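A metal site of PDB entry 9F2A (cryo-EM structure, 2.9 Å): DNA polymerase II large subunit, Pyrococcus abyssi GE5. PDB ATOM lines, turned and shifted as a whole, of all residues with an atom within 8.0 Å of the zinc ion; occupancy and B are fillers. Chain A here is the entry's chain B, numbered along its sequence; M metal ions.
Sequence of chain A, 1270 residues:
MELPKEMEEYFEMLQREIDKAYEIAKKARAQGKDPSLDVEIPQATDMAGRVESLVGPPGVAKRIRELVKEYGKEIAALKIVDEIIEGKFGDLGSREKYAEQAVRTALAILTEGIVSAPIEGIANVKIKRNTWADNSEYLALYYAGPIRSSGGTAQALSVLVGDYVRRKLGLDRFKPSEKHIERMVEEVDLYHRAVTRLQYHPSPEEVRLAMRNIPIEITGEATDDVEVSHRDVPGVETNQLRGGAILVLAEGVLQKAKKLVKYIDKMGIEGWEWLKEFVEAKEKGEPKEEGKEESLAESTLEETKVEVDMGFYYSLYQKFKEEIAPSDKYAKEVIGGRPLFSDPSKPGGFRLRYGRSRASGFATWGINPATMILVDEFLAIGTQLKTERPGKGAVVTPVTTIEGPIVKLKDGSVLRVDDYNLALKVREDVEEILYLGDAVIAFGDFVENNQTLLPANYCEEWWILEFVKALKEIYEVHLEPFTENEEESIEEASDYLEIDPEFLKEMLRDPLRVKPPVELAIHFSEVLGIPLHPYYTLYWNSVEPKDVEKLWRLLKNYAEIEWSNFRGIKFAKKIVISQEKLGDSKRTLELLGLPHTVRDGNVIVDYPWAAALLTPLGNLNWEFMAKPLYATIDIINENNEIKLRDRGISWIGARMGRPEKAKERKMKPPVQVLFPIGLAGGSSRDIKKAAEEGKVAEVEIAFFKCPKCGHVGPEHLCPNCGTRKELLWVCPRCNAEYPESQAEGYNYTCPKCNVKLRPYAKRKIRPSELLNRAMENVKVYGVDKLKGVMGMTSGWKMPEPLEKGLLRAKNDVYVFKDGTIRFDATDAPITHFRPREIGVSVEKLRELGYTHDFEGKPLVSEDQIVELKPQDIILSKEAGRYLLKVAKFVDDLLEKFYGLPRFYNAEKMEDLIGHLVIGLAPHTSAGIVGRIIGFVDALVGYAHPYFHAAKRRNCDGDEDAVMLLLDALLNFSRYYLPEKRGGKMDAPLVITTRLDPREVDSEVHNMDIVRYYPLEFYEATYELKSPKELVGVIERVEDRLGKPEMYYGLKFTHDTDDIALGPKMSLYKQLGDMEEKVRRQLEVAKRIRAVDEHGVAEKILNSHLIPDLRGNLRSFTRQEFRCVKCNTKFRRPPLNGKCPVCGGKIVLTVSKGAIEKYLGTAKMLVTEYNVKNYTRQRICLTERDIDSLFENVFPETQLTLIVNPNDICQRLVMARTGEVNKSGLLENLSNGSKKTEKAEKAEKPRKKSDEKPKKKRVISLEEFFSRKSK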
ATOM      1  N   ARG A1122      -1.839  13.963 -12.971  1.00  0.00           N
ATOM      2  CA  ARG A1122      -2.776  14.171 -11.876  1.00  0.00           C
ATOM      3  C   ARG A1122      -2.464  13.205 -10.735  1.00  0.00           C
ATOM      4  O   ARG A1122      -2.011  12.082 -10.957  1.00  0.00           O
ATOM      5  CB  ARG A1122      -4.217  13.969 -12.357  1.00  0.00           C
ATOM      6  CG  ARG A1122      -5.271  14.299 -11.326  1.00  0.00           C
ATOM      7  CD  ARG A1122      -6.655  13.993 -11.871  1.00  0.00           C
ATOM      8  NE  ARG A1122      -6.873  12.564 -12.033  1.00  0.00           N
ATOM      9  CZ  ARG A1122      -7.599  11.816 -11.223  1.00  0.00           C
ATOM     10  NH1 ARG A1122      -8.199  12.330 -10.158  1.00  0.00           N
ATOM     11  NH2 ARG A1122      -7.731  10.512 -11.469  1.00  0.00           N
ATOM     12  N   CYS A1123      -2.721  13.664  -9.510  1.00  0.00           N
ATOM     13  CA  CYS A1123      -2.659  12.817  -8.336  1.00  0.00           C
ATOM     14  C   CYS A1123      -4.035  12.234  -8.042  1.00  0.00           C
ATOM     15  O   CYS A1123      -5.069  12.798  -8.405  1.00  0.00           O
ATOM     16  CB  CYS A1123      -2.160  13.603  -7.114  1.00  0.00           C
ATOM     17  SG  CYS A1123      -2.139  12.660  -5.554  1.00  0.00           S
ATOM     18  N   VAL A1124      -4.038  11.078  -7.383  1.00  0.00           N
ATOM     19  CA  VAL A1124      -5.287  10.364  -7.161  1.00  0.00           C
ATOM     20  C   VAL A1124      -5.999  10.846  -5.904  1.00  0.00           C
ATOM     21  O   VAL A1124      -7.218  11.033  -5.914  1.00  0.00           O
ATOM     22  CB  VAL A1124      -5.025   8.843  -7.104  1.00  0.00           C
ATOM     23  CG1 VAL A1124      -4.709   8.324  -8.502  1.00  0.00           C
ATOM     24  CG2 VAL A1124      -3.872   8.524  -6.157  1.00  0.00           C
ATOM     25  N   LYS A1125      -5.272  11.060  -4.810  1.00  0.00           N
ATOM     26  CA  LYS A1125      -5.903  11.522  -3.571  1.00  0.00           C
ATOM     27  C   LYS A1125      -6.372  12.966  -3.701  1.00  0.00           C
ATOM     28  O   LYS A1125      -7.562  13.258  -3.541  1.00  0.00           O
ATOM     29  CB  LYS A1125      -4.919  11.362  -2.415  1.00  0.00           C
ATOM     30  CG  LYS A1125      -4.487   9.929  -2.162  1.00  0.00           C
ATOM     31  CD  LYS A1125      -3.381   9.857  -1.117  1.00  0.00           C
ATOM     32  CE  LYS A1125      -3.900  10.245   0.254  1.00  0.00           C
ATOM     33  NZ  LYS A1125      -2.854  10.082   1.302  1.00  0.00           N
ATOM     34  N   CYS A1126      -5.448  13.877  -3.973  1.00  0.00           N
ATOM     35  CA  CYS A1126      -5.808  15.248  -4.298  1.00  0.00           C
ATOM     36  C   CYS A1126      -6.220  15.298  -5.767  1.00  0.00           C
ATOM     37  O   CYS A1126      -6.476  14.269  -6.403  1.00  0.00           O
ATOM     38  CB  CYS A1126      -4.655  16.206  -3.993  1.00  0.00           C
ATOM     39  SG  CYS A1126      -3.246  16.090  -5.140  1.00  0.00           S
ATOM     40  N   ASN A1127      -6.280  16.500  -6.342  1.00  0.00           N
ATOM     41  CA  ASN A1127      -6.519  16.642  -7.772  1.00  0.00           C
ATOM     42  C   ASN A1127      -5.540  17.626  -8.389  1.00  0.00           C
ATOM     43  O   ASN A1127      -5.878  18.337  -9.327  1.00  0.00           O
ATOM     44  CB  ASN A1127      -7.956  17.070  -8.045  1.00  0.00           C
ATOM     45  CG  ASN A1127      -8.910  15.892  -8.069  1.00  0.00           C
ATOM     46  OD1 ASN A1127      -9.064  15.229  -9.097  1.00  0.00           O
ATOM     47  ND2 ASN A1127      -9.564  15.636  -6.949  1.00  0.00           N
ATOM     48  N   THR A1128      -4.316  17.676  -7.870  1.00  0.00           N
ATOM     49  CA  THR A1128      -3.327  18.620  -8.353  1.00  0.00           C
ATOM     50  C   THR A1128      -2.892  18.257  -9.780  1.00  0.00           C
ATOM     51  O   THR A1128      -2.737  17.082 -10.109  1.00  0.00           O
ATOM     52  CB  THR A1128      -2.123  18.655  -7.425  1.00  0.00           C
ATOM     53  OG1 THR A1128      -2.567  18.835  -6.081  1.00  0.00           O
ATOM     54  CG2 THR A1128      -1.188  19.797  -7.796  1.00  0.00           C
ATOM     55  N   LYS A1129      -2.703  19.277 -10.605  1.00  0.00           N
ATOM     56  CA  LYS A1129      -2.252  19.105 -11.976  1.00  0.00           C
ATOM     57  C   LYS A1129      -0.805  19.551 -12.108  1.00  0.00           C
ATOM     58  O   LYS A1129      -0.426  20.611 -11.586  1.00  0.00           O
ATOM     59  CB  LYS A1129      -3.134  19.909 -12.943  1.00  0.00           C
ATOM     60  CG  LYS A1129      -4.602  19.517 -12.920  1.00  0.00           C
ATOM     61  CD  LYS A1129      -4.812  18.154 -13.560  1.00  0.00           C
ATOM     62  CE  LYS A1129      -6.300  17.833 -13.656  1.00  0.00           C
ATOM     63  NZ  LYS A1129      -6.531  16.487 -14.265  1.00  0.00           N
ATOM     64  N   PHE A1130       0.009  18.740 -12.785  1.00  0.00           N
ATOM     65  CA  PHE A1130       1.406  19.035 -13.022  1.00  0.00           C
ATOM     66  C   PHE A1130       1.684  19.043 -14.520  1.00  0.00           C
ATOM     67  O   PHE A1130       1.207  18.156 -15.245  1.00  0.00           O
ATOM     68  CB  PHE A1130       2.320  18.020 -12.335  1.00  0.00           C
ATOM     69  CG  PHE A1130       1.971  17.734 -10.903  1.00  0.00           C
ATOM     70  CD1 PHE A1130       0.968  16.845 -10.589  1.00  0.00           C
ATOM     71  CD2 PHE A1130       2.650  18.353  -9.882  1.00  0.00           C
ATOM     72  CE1 PHE A1130       0.647  16.589  -9.271  1.00  0.00           C
ATOM     73  CE2 PHE A1130       2.329  18.096  -8.564  1.00  0.00           C
ATOM     74  CZ  PHE A1130       1.329  17.212  -8.263  1.00  0.00           C
ATOM     75  N   LYS A1138       5.953  10.392  -7.109  1.00  0.00           N
ATOM     76  CA  LYS A1138       4.883  10.531  -6.134  1.00  0.00           C
ATOM     77  C   LYS A1138       4.456  11.989  -6.051  1.00  0.00           C
ATOM     78  O   LYS A1138       5.132  12.885  -6.553  1.00  0.00           O
ATOM     79  CB  LYS A1138       5.314  10.020  -4.753  1.00  0.00           C
ATOM     80  CG  LYS A1138       5.730   8.558  -4.718  1.00  0.00           C
ATOM     81  CD  LYS A1138       5.506   7.952  -3.352  1.00  0.00           C
ATOM     82  CE  LYS A1138       6.553   6.892  -3.036  1.00  0.00           C
ATOM     83  NZ  LYS A1138       6.679   6.667  -1.567  1.00  0.00           N
ATOM     84  N   CYS A1139       3.317  12.220  -5.406  1.00  0.00           N
ATOM     85  CA  CYS A1139       2.812  13.572  -5.246  1.00  0.00           C
ATOM     86  C   CYS A1139       3.658  14.329  -4.225  1.00  0.00           C
ATOM     87  O   CYS A1139       3.935  13.799  -3.145  1.00  0.00           O
ATOM     88  CB  CYS A1139       1.351  13.543  -4.795  1.00  0.00           C
ATOM     89  SG  CYS A1139       0.559  15.166  -4.676  1.00  0.00           S
ATOM     90  N   PRO A1140       4.090  15.553  -4.543  1.00  0.00           N
ATOM     91  CA  PRO A1140       4.923  16.291  -3.577  1.00  0.00           C
ATOM     92  C   PRO A1140       4.228  16.550  -2.251  1.00  0.00           C
ATOM     93  O   PRO A1140       4.890  16.551  -1.209  1.00  0.00           O
ATOM     94  CB  PRO A1140       5.218  17.600  -4.317  1.00  0.00           C
ATOM     95  CG  PRO A1140       5.097  17.256  -5.760  1.00  0.00           C
ATOM     96  CD  PRO A1140       3.994  16.242  -5.835  1.00  0.00           C
ATOM     97  N   VAL A1141       2.917  16.756  -2.245  1.00  0.00           N
ATOM     98  CA  VAL A1141       2.190  17.071  -1.022  1.00  0.00           C
ATOM     99  C   VAL A1141       1.551  15.803  -0.470  1.00  0.00           C
ATOM    100  O   VAL A1141       1.825  15.394   0.664  1.00  0.00           O
ATOM    101  CB  VAL A1141       1.137  18.161  -1.261  1.00  0.00           C
ATOM    102  CG1 VAL A1141       0.375  18.461   0.017  1.00  0.00           C
ATOM    103  CG2 VAL A1141       1.804  19.424  -1.800  1.00  0.00           C
ATOM    104  N   CYS A1142       0.671  15.181  -1.265  1.00  0.00           N
ATOM    105  CA  CYS A1142      -0.025  13.985  -0.810  1.00  0.00           C
ATOM    106  C   CYS A1142       0.940  12.841  -0.563  1.00  0.00           C
ATOM    107  O   CYS A1142       0.828  12.125   0.438  1.00  0.00           O
ATOM    108  CB  CYS A1142      -1.073  13.573  -1.844  1.00  0.00           C
ATOM    109  SG  CYS A1142      -2.383  14.753  -2.122  1.00  0.00           S
ATOM    110  N   GLY A1143       1.893  12.648  -1.467  1.00  0.00           N
ATOM    111  CA  GLY A1143       2.632  11.398  -1.510  1.00  0.00           C
ATOM    112  C   GLY A1143       1.933  10.295  -2.250  1.00  0.00           C
ATOM    113  O   GLY A1143       2.450   9.169  -2.289  1.00  0.00           O
ATOM    114  N   GLY A1144       0.769  10.572  -2.841  1.00  0.00           N
ATOM    115  CA  GLY A1144      -0.003   9.565  -3.528  1.00  0.00           C
ATOM    116  C   GLY A1144       0.463   9.330  -4.953  1.00  0.00           C
ATOM    117  O   GLY A1144       1.430   9.917  -5.440  1.00  0.00           O
ATOM    118  N   LYS A1145      -0.247   8.442  -5.634  1.00  0.00           N
ATOM    119  CA  LYS A1145       0.133   7.995  -6.964  1.00  0.00           C
ATOM    120  C   LYS A1145      -0.188   9.046  -8.012  1.00  0.00           C
ATOM    121  O   LYS A1145      -1.198   9.751  -7.915  1.00  0.00           O
ATOM    122  CB  LYS A1145      -0.571   6.681  -7.300  1.00  0.00           C
ATOM    123  CG  LYS A1145      -0.050   5.981  -8.534  1.00  0.00           C
ATOM    124  CD  LYS A1145      -0.744   4.644  -8.746  1.00  0.00           C
ATOM    125  CE  LYS A1145      -0.321   3.626  -7.702  1.00  0.00           C
ATOM    126  NZ  LYS A1145       1.117   3.250  -7.831  1.00  0.00           N
ATOM    127  N   ILE A1146       0.670   9.149  -9.019  1.00  0.00           N
ATOM    128  CA  ILE A1146       0.492  10.054 -10.148  1.00  0.00           C
ATOM    129  C   ILE A1146       0.056   9.234 -11.352  1.00  0.00           C
ATOM    130  O   ILE A1146       0.678   8.207 -11.670  1.00  0.00           O
ATOM    131  CB  ILE A1146       1.784  10.837 -10.452  1.00  0.00           C
ATOM    132  CG1 ILE A1146       2.014  11.895  -9.372  1.00  0.00           C
ATOM    133  CG2 ILE A1146       1.703  11.488 -11.814  1.00  0.00           C
ATOM    134  CD1 ILE A1146       1.025  13.034  -9.422  1.00  0.00           C
HETATM  135 ZN    ZN M   1      -1.673  14.587  -4.335  1.00  0.00          ZN
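The zinc ion is bound by SG of Cys 1126, at 2.3 Å. The zinc ion is bound by the side-chain sulfur (SG) of Cys 1123 (2.3 Å). SG of Cys 1142 is bound to the zinc ion, 2.3 Å away. SG of Cys 1139 binds the zinc ion (2.3 Å). The zinc ion has four donor atoms within binding distance.
N of Cys 1139 lies within hydrogen-bond range of O of Gly 1144, at 3.0 Å. The side-chain sulfur (SG) of Cys 1123 sits close to the backbone NH (N) of Lys 1125, at 3.6 Å. OG1 of Thr 1128 lies close to SG of Cys 1126 (3.0 Å). SG of Cys 1139 lies close to N of Val 1141, 3.7 Å away. The backbone NH (N) of Cys 1123 sits at hydrogen-bond distance from the backbone carbonyl oxygen (O) of Thr 1128 (3.5 Å).
Four residues have an atom within 4 Å of the zinc ion: Cys 1123, Cys 1126, Cys 1139 and Cys 1142.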
